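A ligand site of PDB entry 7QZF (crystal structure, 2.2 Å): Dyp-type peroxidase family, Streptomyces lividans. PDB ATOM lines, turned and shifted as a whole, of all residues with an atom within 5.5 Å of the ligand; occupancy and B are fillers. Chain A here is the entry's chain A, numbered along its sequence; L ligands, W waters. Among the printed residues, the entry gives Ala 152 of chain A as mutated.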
ATOM      1  N   ASP A 146       7.645 -15.276 -16.317  1.00  0.00           N
ATOM      2  CA  ASP A 146       8.481 -16.462 -16.584  1.00  0.00           C
ATOM      3  C   ASP A 146       7.598 -17.709 -16.457  1.00  0.00           C
ATOM      4  O   ASP A 146       6.398 -17.599 -16.270  1.00  0.00           O
ATOM      5  CB  ASP A 146       9.695 -16.503 -15.639  1.00  0.00           C
ATOM      6  CG  ASP A 146       9.386 -16.742 -14.159  1.00  0.00           C
ATOM      7  OD1 ASP A 146       8.227 -17.157 -13.847  1.00  0.00           O
ATOM      8  OD2 ASP A 146      10.358 -16.493 -13.324  1.00  0.00           O
ATOM      9  N   LEU A 148       7.228 -19.877 -14.192  1.00  0.00           N
ATOM     10  CA  LEU A 148       6.594 -20.044 -12.868  1.00  0.00           C
ATOM     11  C   LEU A 148       5.422 -19.085 -12.669  1.00  0.00           C
ATOM     12  O   LEU A 148       4.702 -19.240 -11.636  1.00  0.00           O
ATOM     13  CB  LEU A 148       7.629 -19.888 -11.764  1.00  0.00           C
ATOM     14  CG  LEU A 148       8.823 -20.857 -11.894  1.00  0.00           C
ATOM     15  CD1 LEU A 148       9.846 -20.679 -10.787  1.00  0.00           C
ATOM     16  CD2 LEU A 148       8.310 -22.299 -12.004  1.00  0.00           C
ATOM     17  N   PHE A 150       5.753 -15.697 -12.391  1.00  0.00           N
ATOM     18  CA  PHE A 150       6.272 -14.452 -11.734  1.00  0.00           C
ATOM     19  C   PHE A 150       6.918 -13.527 -12.797  1.00  0.00           C
ATOM     20  O   PHE A 150       7.478 -14.019 -13.786  1.00  0.00           O
ATOM     21  CB  PHE A 150       7.244 -14.807 -10.606  1.00  0.00           C
ATOM     22  CG  PHE A 150       6.486 -15.269  -9.365  1.00  0.00           C
ATOM     23  CD1 PHE A 150       5.832 -16.492  -9.363  1.00  0.00           C
ATOM     24  CD2 PHE A 150       6.437 -14.501  -8.221  1.00  0.00           C
ATOM     25  CE1 PHE A 150       5.155 -16.948  -8.236  1.00  0.00           C
ATOM     26  CE2 PHE A 150       5.750 -14.932  -7.113  1.00  0.00           C
ATOM     27  CZ  PHE A 150       5.102 -16.147  -7.109  1.00  0.00           C
ATOM     28  N   VAL A 151       6.876 -12.212 -12.540  1.00  0.00           N
ATOM     29  CA  VAL A 151       7.568 -11.211 -13.384  1.00  0.00           C
ATOM     30  C   VAL A 151       9.056 -11.457 -13.251  1.00  0.00           C
ATOM     31  O   VAL A 151       9.529 -11.621 -12.079  1.00  0.00           O
ATOM     32  CB  VAL A 151       7.149  -9.767 -13.011  1.00  0.00           C
ATOM     33  CG1 VAL A 151       7.904  -8.725 -13.855  1.00  0.00           C
ATOM     34  CG2 VAL A 151       5.662  -9.545 -13.202  1.00  0.00           C
ATOM     35  N   ALA A 152       9.788 -11.484 -14.364  1.00  0.00           N
ATOM     36  CA  ALA A 152      11.257 -11.701 -14.384  1.00  0.00           C
ATOM     37  C   ALA A 152      11.958 -10.449 -14.937  1.00  0.00           C
ATOM     38  O   ALA A 152      11.667 -10.084 -16.077  1.00  0.00           O
ATOM     39  CB  ALA A 152      11.495 -12.915 -15.259  1.00  0.00           C
ATOM     40  N   GLY A 153      12.873  -9.845 -14.213  1.00  0.00           N
ATOM     41  CA  GLY A 153      13.760  -8.748 -14.712  1.00  0.00           C
ATOM     42  C   GLY A 153      13.653  -7.478 -13.894  1.00  0.00           C
ATOM     43  O   GLY A 153      14.536  -6.632 -14.008  1.00  0.00           O
ATOM     44  N   THR A 154      12.691  -7.425 -13.000  1.00  0.00           N
ATOM     45  CA  THR A 154      12.286  -6.237 -12.226  1.00  0.00           C
ATOM     46  C   THR A 154      13.466  -5.534 -11.577  1.00  0.00           C
ATOM     47  O   THR A 154      13.550  -4.280 -11.754  1.00  0.00           O
ATOM     48  CB  THR A 154      11.279  -6.573 -11.138  1.00  0.00           C
ATOM     49  OG1 THR A 154      10.267  -7.374 -11.758  1.00  0.00           O
ATOM     50  CG2 THR A 154      10.702  -5.312 -10.531  1.00  0.00           C
ATOM     51  N   GLU A 155      14.332  -6.265 -10.863  1.00  0.00           N
ATOM     52  CA  GLU A 155      15.399  -5.593 -10.059  1.00  0.00           C
ATOM     53  C   GLU A 155      16.744  -5.553 -10.802  1.00  0.00           C
ATOM     54  O   GLU A 155      17.741  -5.259 -10.172  1.00  0.00           O
ATOM     55  CB  GLU A 155      15.571  -6.209  -8.684  1.00  0.00           C
ATOM     56  CG  GLU A 155      14.463  -5.818  -7.721  1.00  0.00           C
ATOM     57  CD  GLU A 155      14.323  -4.337  -7.423  1.00  0.00           C
ATOM     58  OE1 GLU A 155      15.175  -3.807  -6.727  1.00  0.00           O
ATOM     59  OE2 GLU A 155      13.331  -3.771  -7.823  1.00  0.00           O
ATOM     60  N   ASN A 156      16.787  -5.868 -12.094  1.00  0.00           N
ATOM     61  CA  ASN A 156      18.005  -5.623 -12.908  1.00  0.00           C
ATOM     62  C   ASN A 156      18.444  -4.184 -12.719  1.00  0.00           C
ATOM     63  O   ASN A 156      17.610  -3.294 -12.699  1.00  0.00           O
ATOM     64  CB  ASN A 156      17.798  -5.902 -14.395  1.00  0.00           C
ATOM     65  CG  ASN A 156      18.097  -7.325 -14.792  1.00  0.00           C
ATOM     66  OD1 ASN A 156      18.965  -8.000 -14.201  1.00  0.00           O
ATOM     67  ND2 ASN A 156      17.404  -7.795 -15.793  1.00  0.00           N
ATOM     68  N   GLN A 184      22.795 -21.281 -17.571  1.00  0.00           N
ATOM     69  CA  GLN A 184      22.239 -22.564 -17.029  1.00  0.00           C
ATOM     70  C   GLN A 184      20.863 -22.788 -17.663  1.00  0.00           C
ATOM     71  O   GLN A 184      19.970 -21.926 -17.467  1.00  0.00           O
ATOM     72  CB  GLN A 184      22.105 -22.463 -15.492  1.00  0.00           C
ATOM     73  CG  GLN A 184      23.436 -22.420 -14.725  1.00  0.00           C
ATOM     74  CD  GLN A 184      23.144 -22.421 -13.215  1.00  0.00           C
ATOM     75  OE1 GLN A 184      22.525 -21.548 -12.679  1.00  0.00           O
ATOM     76  NE2 GLN A 184      23.465 -23.499 -12.532  1.00  0.00           N
ATOM     77  N   TYR A 186      17.496 -24.578 -17.046  1.00  0.00           N
ATOM     78  CA  TYR A 186      16.706 -25.182 -15.958  1.00  0.00           C
ATOM     79  C   TYR A 186      15.459 -25.782 -16.606  1.00  0.00           C
ATOM     80  O   TYR A 186      14.825 -25.126 -17.515  1.00  0.00           O
ATOM     81  CB  TYR A 186      16.363 -24.140 -14.904  1.00  0.00           C
ATOM     82  CG  TYR A 186      17.474 -23.703 -13.962  1.00  0.00           C
ATOM     83  CD1 TYR A 186      17.714 -24.387 -12.778  1.00  0.00           C
ATOM     84  CD2 TYR A 186      18.232 -22.559 -14.217  1.00  0.00           C
ATOM     85  CE1 TYR A 186      18.695 -23.995 -11.877  1.00  0.00           C
ATOM     86  CE2 TYR A 186      19.269 -22.188 -13.354  1.00  0.00           C
ATOM     87  CZ  TYR A 186      19.478 -22.877 -12.152  1.00  0.00           C
ATOM     88  OH  TYR A 186      20.498 -22.521 -11.280  1.00  0.00           O
ATOM     89  N   HIS A 188      11.637 -27.104 -15.066  1.00  0.00           N
ATOM     90  CA  HIS A 188      10.737 -26.960 -13.915  1.00  0.00           C
ATOM     91  C   HIS A 188       9.851 -28.202 -13.797  1.00  0.00           C
ATOM     92  O   HIS A 188       9.438 -28.770 -14.800  1.00  0.00           O
ATOM     93  CB  HIS A 188       9.918 -25.642 -13.956  1.00  0.00           C
ATOM     94  CG  HIS A 188      10.794 -24.451 -13.948  1.00  0.00           C
ATOM     95  ND1 HIS A 188      11.560 -24.125 -12.854  1.00  0.00           N
ATOM     96  CD2 HIS A 188      11.043 -23.505 -14.908  1.00  0.00           C
ATOM     97  CE1 HIS A 188      12.257 -23.001 -13.147  1.00  0.00           C
ATOM     98  NE2 HIS A 188      11.944 -22.603 -14.403  1.00  0.00           N
ATOM     99  N   ILE A 205       9.622 -17.328  -3.779  1.00  0.00           N
ATOM    100  CA  ILE A 205      10.269 -16.283  -4.612  1.00  0.00           C
ATOM    101  C   ILE A 205      10.750 -15.091  -3.740  1.00  0.00           C
ATOM    102  O   ILE A 205      11.898 -14.665  -3.860  1.00  0.00           O
ATOM    103  CB  ILE A 205       9.309 -15.859  -5.746  1.00  0.00           C
ATOM    104  CG1 ILE A 205       8.910 -17.045  -6.639  1.00  0.00           C
ATOM    105  CG2 ILE A 205       9.897 -14.682  -6.567  1.00  0.00           C
ATOM    106  CD1 ILE A 205      10.050 -17.613  -7.410  1.00  0.00           C
ATOM    107  N   ARG A 207       8.439 -12.259  -3.541  1.00  0.00           N
ATOM    108  CA  ARG A 207       7.672 -11.113  -4.117  1.00  0.00           C
ATOM    109  C   ARG A 207       6.233 -11.590  -4.328  1.00  0.00           C
ATOM    110  O   ARG A 207       6.044 -12.826  -4.457  1.00  0.00           O
ATOM    111  CB  ARG A 207       8.253 -10.557  -5.444  1.00  0.00           C
ATOM    112  CG  ARG A 207       9.773 -10.381  -5.495  1.00  0.00           C
ATOM    113  CD  ARG A 207      10.302  -9.871  -6.840  1.00  0.00           C
ATOM    114  NE  ARG A 207       9.797  -8.520  -7.095  1.00  0.00           N
ATOM    115  CZ  ARG A 207      10.393  -7.388  -6.722  1.00  0.00           C
ATOM    116  NH1 ARG A 207      11.602  -7.375  -6.175  1.00  0.00           N
ATOM    117  NH2 ARG A 207       9.776  -6.242  -6.998  1.00  0.00           N
ATOM    118  N   ASP A 212       3.921  -7.968  -8.066  1.00  0.00           N
ATOM    119  CA  ASP A 212       5.389  -7.867  -8.173  1.00  0.00           C
ATOM    120  C   ASP A 212       5.962  -6.913  -7.098  1.00  0.00           C
ATOM    121  O   ASP A 212       7.049  -6.389  -7.267  1.00  0.00           O
ATOM    122  CB  ASP A 212       5.809  -7.447  -9.587  1.00  0.00           C
ATOM    123  CG  ASP A 212       7.280  -7.737  -9.930  1.00  0.00           C
ATOM    124  OD1 ASP A 212       7.864  -8.645  -9.242  1.00  0.00           O
ATOM    125  OD2 ASP A 212       7.812  -7.105 -10.860  1.00  0.00           O
ATOM    126  N   GLU A 214       7.835  -6.517  -3.642  1.00  0.00           N
ATOM    127  CA  GLU A 214       8.753  -7.308  -2.800  1.00  0.00           C
ATOM    128  C   GLU A 214       8.081  -7.533  -1.437  1.00  0.00           C
ATOM    129  O   GLU A 214       7.452  -6.627  -0.951  1.00  0.00           O
ATOM    130  CB  GLU A 214      10.089  -6.549  -2.676  1.00  0.00           C
ATOM    131  CG  GLU A 214      11.141  -7.412  -2.001  1.00  0.00           C
ATOM    132  CD  GLU A 214      12.558  -6.943  -2.087  1.00  0.00           C
ATOM    133  OE1 GLU A 214      12.898  -6.274  -3.093  1.00  0.00           O
ATOM    134  OE2 GLU A 214      13.314  -7.239  -1.142  1.00  0.00           O
ATOM    135  N   HIS A 225      14.146 -16.992  -2.796  1.00  0.00           N
ATOM    136  CA  HIS A 225      15.085 -16.783  -3.890  1.00  0.00           C
ATOM    137  C   HIS A 225      15.670 -15.378  -3.796  1.00  0.00           C
ATOM    138  O   HIS A 225      16.893 -15.236  -3.983  1.00  0.00           O
ATOM    139  CB  HIS A 225      14.394 -17.042  -5.215  1.00  0.00           C
ATOM    140  CG  HIS A 225      15.287 -16.818  -6.380  1.00  0.00           C
ATOM    141  ND1 HIS A 225      16.465 -17.520  -6.549  1.00  0.00           N
ATOM    142  CD2 HIS A 225      15.134 -16.001  -7.445  1.00  0.00           C
ATOM    143  CE1 HIS A 225      16.978 -17.175  -7.705  1.00  0.00           C
ATOM    144  NE2 HIS A 225      16.168 -16.226  -8.283  1.00  0.00           N
ATOM    145  N   VAL A 226      14.838 -14.365  -3.521  1.00  0.00           N
ATOM    146  CA  VAL A 226      15.322 -12.945  -3.482  1.00  0.00           C
ATOM    147  C   VAL A 226      16.281 -12.714  -2.296  1.00  0.00           C
ATOM    148  O   VAL A 226      17.211 -11.974  -2.441  1.00  0.00           O
ATOM    149  CB  VAL A 226      14.099 -11.996  -3.491  1.00  0.00           C
ATOM    150  CG1 VAL A 226      14.461 -10.606  -2.982  1.00  0.00           C
ATOM    151  CG2 VAL A 226      13.559 -11.960  -4.912  1.00  0.00           C
ATOM    152  N   THR A 229      19.815 -14.318  -3.249  1.00  0.00           N
ATOM    153  CA  THR A 229      20.564 -13.708  -4.391  1.00  0.00           C
ATOM    154  C   THR A 229      20.805 -12.229  -4.114  1.00  0.00           C
ATOM    155  O   THR A 229      21.340 -11.536  -4.993  1.00  0.00           O
ATOM    156  CB  THR A 229      19.858 -14.003  -5.728  1.00  0.00           C
ATOM    157  OG1 THR A 229      18.522 -13.500  -5.667  1.00  0.00           O
ATOM    158  CG2 THR A 229      19.834 -15.493  -6.006  1.00  0.00           C
ATOM    159  N   SER A 230      20.404 -11.738  -2.943  1.00  0.00           N
ATOM    160  CA  SER A 230      20.777 -10.378  -2.452  1.00  0.00           C
ATOM    161  C   SER A 230      22.109 -10.466  -1.725  1.00  0.00           C
ATOM    162  O   SER A 230      22.184 -11.304  -0.796  1.00  0.00           O
ATOM    163  CB  SER A 230      19.698  -9.797  -1.612  1.00  0.00           C
ATOM    164  OG  SER A 230      18.571  -9.548  -2.471  1.00  0.00           O
ATOM    165  N   ILE A 241      24.180  -8.202 -10.752  1.00  0.00           N
ATOM    166  CA  ILE A 241      24.426  -8.744 -12.109  1.00  0.00           C
ATOM    167  C   ILE A 241      23.257  -8.296 -13.020  1.00  0.00           C
ATOM    168  O   ILE A 241      22.228  -7.865 -12.544  1.00  0.00           O
ATOM    169  CB  ILE A 241      24.563 -10.272 -12.073  1.00  0.00           C
ATOM    170  CG1 ILE A 241      23.224 -10.941 -11.693  1.00  0.00           C
ATOM    171  CG2 ILE A 241      25.698 -10.713 -11.138  1.00  0.00           C
ATOM    172  CD1 ILE A 241      23.284 -12.480 -11.732  1.00  0.00           C
ATOM    173  N   ARG A 243      20.628  -9.874 -15.735  1.00  0.00           N
ATOM    174  CA  ARG A 243      19.988 -11.166 -16.103  1.00  0.00           C
ATOM    175  C   ARG A 243      19.060 -10.995 -17.299  1.00  0.00           C
ATOM    176  O   ARG A 243      18.481  -9.883 -17.453  1.00  0.00           O
ATOM    177  CB  ARG A 243      19.204 -11.684 -14.917  1.00  0.00           C
ATOM    178  CG  ARG A 243      20.039 -11.927 -13.671  1.00  0.00           C
ATOM    179  CD  ARG A 243      19.231 -12.086 -12.408  1.00  0.00           C
ATOM    180  NE  ARG A 243      18.624 -10.809 -11.979  1.00  0.00           N
ATOM    181  CZ  ARG A 243      17.313 -10.545 -12.006  1.00  0.00           C
ATOM    182  NH1 ARG A 243      16.429 -11.472 -12.368  1.00  0.00           N
ATOM    183  NH2 ARG A 243      16.881  -9.362 -11.629  1.00  0.00           N
ATOM    184  N   THR A 258      13.397 -22.574 -17.998  1.00  0.00           N
ATOM    185  CA  THR A 258      13.951 -21.217 -17.976  1.00  0.00           C
ATOM    186  C   THR A 258      15.373 -21.332 -18.449  1.00  0.00           C
ATOM    187  O   THR A 258      16.154 -22.107 -17.812  1.00  0.00           O
ATOM    188  CB  THR A 258      13.956 -20.643 -16.538  1.00  0.00           C
ATOM    189  OG1 THR A 258      12.624 -20.460 -16.093  1.00  0.00           O
ATOM    190  CG2 THR A 258      14.630 -19.277 -16.409  1.00  0.00           C
ATOM    191  N   PHE A 260      18.608 -19.535 -18.116  1.00  0.00           N
ATOM    192  CA  PHE A 260      19.198 -18.457 -17.320  1.00  0.00           C
ATOM    193  C   PHE A 260      20.491 -17.984 -17.999  1.00  0.00           C
ATOM    194  O   PHE A 260      21.367 -18.850 -18.330  1.00  0.00           O
ATOM    195  CB  PHE A 260      19.494 -18.927 -15.887  1.00  0.00           C
ATOM    196  CG  PHE A 260      20.235 -17.901 -15.091  1.00  0.00           C
ATOM    197  CD1 PHE A 260      19.547 -16.890 -14.435  1.00  0.00           C
ATOM    198  CD2 PHE A 260      21.607 -17.923 -15.034  1.00  0.00           C
ATOM    199  CE1 PHE A 260      20.239 -15.907 -13.725  1.00  0.00           C
ATOM    200  CE2 PHE A 260      22.294 -16.914 -14.357  1.00  0.00           C
ATOM    201  CZ  PHE A 260      21.618 -15.925 -13.702  1.00  0.00           C
ATOM    202  N   THR A 270      28.608 -13.657  -9.602  1.00  0.00           N
ATOM    203  CA  THR A 270      27.632 -14.704 -10.017  1.00  0.00           C
ATOM    204  C   THR A 270      27.873 -15.992  -9.229  1.00  0.00           C
ATOM    205  O   THR A 270      26.877 -16.624  -8.863  1.00  0.00           O
ATOM    206  CB  THR A 270      27.643 -14.990 -11.526  1.00  0.00           C
ATOM    207  OG1 THR A 270      27.656 -13.739 -12.223  1.00  0.00           O
ATOM    208  CG2 THR A 270      26.417 -15.782 -11.940  1.00  0.00           C
ATOM    209  N   MET A 273      26.448 -15.896  -5.604  1.00  0.00           N
ATOM    210  CA  MET A 273      24.989 -16.122  -5.687  1.00  0.00           C
ATOM    211  C   MET A 273      24.692 -17.596  -5.865  1.00  0.00           C
ATOM    212  O   MET A 273      23.739 -18.081  -5.153  1.00  0.00           O
ATOM    213  CB  MET A 273      24.322 -15.313  -6.789  1.00  0.00           C
ATOM    214  CG  MET A 273      24.382 -13.806  -6.537  1.00  0.00           C
ATOM    215  SD  MET A 273      23.791 -12.956  -7.974  1.00  0.00           S
ATOM    216  CE  MET A 273      24.023 -11.266  -7.397  1.00  0.00           C
ATOM    217  N   LEU A 274      25.400 -18.286  -6.775  1.00  0.00           N
ATOM    218  CA  LEU A 274      25.169 -19.746  -7.056  1.00  0.00           C
ATOM    219  C   LEU A 274      25.511 -20.600  -5.812  1.00  0.00           C
ATOM    220  O   LEU A 274      24.687 -21.514  -5.507  1.00  0.00           O
ATOM    221  CB  LEU A 274      26.026 -20.182  -8.243  1.00  0.00           C
ATOM    222  CG  LEU A 274      25.514 -19.755  -9.621  1.00  0.00           C
ATOM    223  CD1 LEU A 274      26.582 -19.886 -10.677  1.00  0.00           C
ATOM    224  CD2 LEU A 274      24.339 -20.621 -10.006  1.00  0.00           C
ATOM    225  N   MET A 277      22.698 -20.214  -3.329  1.00  0.00           N
ATOM    226  CA  MET A 277      21.491 -20.972  -3.835  1.00  0.00           C
ATOM    227  C   MET A 277      21.662 -22.467  -3.575  1.00  0.00           C
ATOM    228  O   MET A 277      20.770 -23.047  -2.973  1.00  0.00           O
ATOM    229  CB  MET A 277      21.239 -20.739  -5.326  1.00  0.00           C
ATOM    230  CG  MET A 277      20.693 -19.353  -5.644  1.00  0.00           C
ATOM    231  SD  MET A 277      20.568 -19.168  -7.471  1.00  0.00           S
ATOM    232  CE  MET A 277      19.286 -20.338  -7.856  1.00  0.00           C
ATOM    233  N   ILE A 289      13.619 -22.317  -4.690  1.00  0.00           N
ATOM    234  CA  ILE A 289      13.323 -22.380  -6.151  1.00  0.00           C
ATOM    235  C   ILE A 289      13.911 -23.657  -6.723  1.00  0.00           C
ATOM    236  O   ILE A 289      13.344 -24.205  -7.695  1.00  0.00           O
ATOM    237  CB  ILE A 289      13.783 -21.095  -6.859  1.00  0.00           C
ATOM    238  CG1 ILE A 289      12.898 -20.727  -8.052  1.00  0.00           C
ATOM    239  CG2 ILE A 289      15.239 -21.114  -7.261  1.00  0.00           C
ATOM    240  CD1 ILE A 289      13.262 -19.427  -8.737  1.00  0.00           C
ATOM    241  N   SER A 293      13.080 -26.780  -9.771  1.00  0.00           N
ATOM    242  CA  SER A 293      13.968 -26.334 -10.885  1.00  0.00           C
ATOM    243  C   SER A 293      15.258 -27.136 -10.847  1.00  0.00           C
ATOM    244  O   SER A 293      15.954 -27.092  -9.801  1.00  0.00           O
ATOM    245  CB  SER A 293      14.305 -24.835 -10.821  1.00  0.00           C
ATOM    246  OG  SER A 293      13.197 -24.038 -10.432  1.00  0.00           O
HETATM  247  C1  LIG L   1      15.362 -12.221  -9.016  1.00  0.00           C
HETATM  248  C2  LIG L   1      13.260 -16.096 -11.215  1.00  0.00           C
HETATM  249  C3  LIG L   1      17.570 -18.375 -11.309  1.00  0.00           C
HETATM  250  C4  LIG L   1      19.724 -14.340  -9.679  1.00  0.00           C
HETATM  251  C5  LIG L   1      14.455 -13.115  -9.584  1.00  0.00           C
HETATM  252  C6  LIG L   1      13.045 -12.923  -9.594  1.00  0.00           C
HETATM  253  C7  LIG L   1      12.448 -13.954 -10.250  1.00  0.00           C
HETATM  254  C8  LIG L   1      13.450 -14.869 -10.562  1.00  0.00           C
HETATM  255  C9  LIG L   1      10.977 -14.126 -10.453  1.00  0.00           C
HETATM  256  C10 LIG L   1      12.374 -11.660  -9.015  1.00  0.00           C
HETATM  257  C11 LIG L   1      12.230 -10.478  -9.929  1.00  0.00           C
HETATM  258  C12 LIG L   1      13.563  -9.879 -10.468  1.00  0.00           C
HETATM  259  O1  LIG L   1      13.979 -10.345 -11.528  1.00  0.00           O
HETATM  260  O2  LIG L   1      14.204  -8.958  -9.912  1.00  0.00           O
HETATM  261  C13 LIG L   1      14.277 -17.036 -11.429  1.00  0.00           C
HETATM  262  C14 LIG L   1      13.958 -18.332 -12.031  1.00  0.00           C
HETATM  263  C15 LIG L   1      15.176 -18.966 -12.133  1.00  0.00           C
HETATM  264  C16 LIG L   1      16.223 -18.090 -11.465  1.00  0.00           C
HETATM  265  C17 LIG L   1      12.579 -18.833 -12.627  1.00  0.00           C
HETATM  266  C18 LIG L   1      15.189 -20.313 -12.628  1.00  0.00           C
HETATM  267  C19 LIG L   1      16.022 -21.187 -12.157  1.00  0.00           C
HETATM  268  C20 LIG L   1      18.572 -17.481 -10.871  1.00  0.00           C
HETATM  269  C21 LIG L   1      19.961 -17.753 -10.791  1.00  0.00           C
HETATM  270  C22 LIG L   1      20.532 -16.599 -10.285  1.00  0.00           C
HETATM  271  C23 LIG L   1      19.520 -15.582 -10.185  1.00  0.00           C
HETATM  272  C24 LIG L   1      20.638 -19.030 -11.033  1.00  0.00           C
HETATM  273  C25 LIG L   1      21.955 -16.291  -9.968  1.00  0.00           C
HETATM  274  C26 LIG L   1      22.968 -17.039 -10.168  1.00  0.00           C
HETATM  275  C27 LIG L   1      18.698 -13.472  -9.360  1.00  0.00           C
HETATM  276  C28 LIG L   1      18.944 -12.176  -8.839  1.00  0.00           C
HETATM  277  C29 LIG L   1      17.755 -11.564  -8.642  1.00  0.00           C
HETATM  278  C30 LIG L   1      16.739 -12.539  -9.022  1.00  0.00           C
HETATM  279  C31 LIG L   1      20.236 -11.487  -8.563  1.00  0.00           C
HETATM  280  C32 LIG L   1      17.599 -10.162  -8.090  1.00  0.00           C
HETATM  281  C33 LIG L   1      17.196 -10.205  -6.637  1.00  0.00           C
HETATM  282  C34 LIG L   1      17.184  -8.853  -5.967  1.00  0.00           C
HETATM  283  O3  LIG L   1      18.278  -8.522  -5.611  1.00  0.00           O
HETATM  284  O4  LIG L   1      16.238  -8.101  -5.636  1.00  0.00           O
HETATM  285  N1  LIG L   1      14.673 -14.346 -10.186  1.00  0.00           N
HETATM  286  N2  LIG L   1      15.590 -16.942 -11.102  1.00  0.00           N
HETATM  287  N3  LIG L   1      18.340 -16.168 -10.444  1.00  0.00           N
HETATM  288  N4  LIG L   1      17.342 -13.657  -9.510  1.00  0.00           N
HETATM  289 FE1  LIG L   1      16.465 -15.262 -10.202  1.00  0.00          FE
HETATM  290  O   HOH W   1      12.843 -15.865 -14.543  1.00  0.00           O
HETATM  291  O   HOH W   2      15.664  -5.716  -4.520  1.00  0.00           O
HETATM  292  O   HOH W   3      20.714  -9.157  -6.473  1.00  0.00           O
HETATM  293  O   HOH W   4      16.401 -14.654 -12.899  1.00  0.00           O
HETATM  294  O   HOH W   5      13.759  -9.266  -7.367  1.00  0.00           O
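NE2 of His 225 is bound to FE1 of the ligand. NH1 of Arg 243 is in salt-bridge range of O1 of the ligand, 2.8 Å away. The backbone NH (N) of Glu 155 lies within hydrogen-bond range of an oxygen (O2) of the ligand. The backbone NH (N) of Gly 153 sits at hydrogen-bond distance from an oxygen (O1) of the ligand, at 2.9 Å. The side-chain hydroxyl (OG) of Ser 230 is in hydrogen-bond range of an oxygen (O3) of the ligand (3.3 Å).
The side-chain hydroxyl of Thr 229 is in hydrogen-bond range of the backbone carbonyl oxygen of His 225. The backbone NH (N) of His 225 lies within hydrogen-bond range of the backbone carbonyl oxygen (O) of Ile 205 (3.4 Å). N of Leu 148 sits at hydrogen-bond distance from OD1 of Asp 146, 2.9 Å away. OD1 of Asp 146 lies within hydrogen-bond range of N of Phe 150, at 3.2 Å. The side-chain hydroxyl (OH) of Tyr 186 is in hydrogen-bond range of the side-chain amide oxygen (OE1) of Gln 184. The backbone NH of Tyr 186 is in hydrogen-bond range of the backbone carbonyl oxygen of Thr 258 (2.9 Å). The backbone NH (N) of Phe 260 sits at hydrogen-bond distance from the backbone carbonyl oxygen (O) of Gln 184 (2.8 Å). The side-chain carboxylate (OD2) of Asp 212 lies within hydrogen-bond range of the side-chain hydroxyl (OG1) of Thr 154, 2.6 Å away.
Asp 146 touches the ligand (OD2 to C17, 3.3 Å). CD1 of Leu 148 touches C17 of the ligand, at 3.8 Å. Phe 150 touches the ligand. Val 151 touches the ligand. Ala 152 touches the ligand (C to O1, 3.96 Å). N of Thr 154 touches O1 of the ligand, at 3.5 Å. Gln 184 touches the ligand. CD2 of Tyr 186 touches C19 of the ligand, at 3.3 Å. Arg 207 touches the ligand (CD to C10, 3.5 Å). OG1 of Thr 229 touches C28 of the ligand, 3.5 Å away. OG1 of Thr 258 touches C17 of the ligand, 3.8 Å away. Phe 260 touches the ligand. Met 273 touches the ligand. Leu 274 touches the ligand. SD of Met 277 touches C24 of the ligand, 3.6 Å away. Ile 289 touches the ligand. Hydrophobic or aromatic side chains that line the ligand: Leu 148, Phe 150, Tyr 186, His 225, Phe 260, Met 273, Leu 274, Met 277 and Ile 289. Within 4 Å of the ligand: Asp 146, Leu 148, Phe 150, Val 151, Ala 152, Gly 153, Thr 154, Glu 155, Gln 184, Tyr 186, Arg 207, His 225, Thr 229, Ser 230, Arg 243, Thr 258, Phe 260, Met 273, Leu 274, Met 277 and Ile 289. The nearest printed residue that does not touch the ligand is His 188 (4.01 Å).
Water W5 bridges an oxygen (O2) of the ligand (2.6 Å) and the guanidinium group (NH1) of Arg 207 (3.1 Å). Water W3 lies within hydrogen-bond range of O3 of the ligand and O of Thr 229. Water W2 lies within hydrogen-bond range of O4 of the ligand (2.7 Å), OE1 of Glu 155 (3.0 Å) and OE1 of Glu 214 (3.2 Å).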
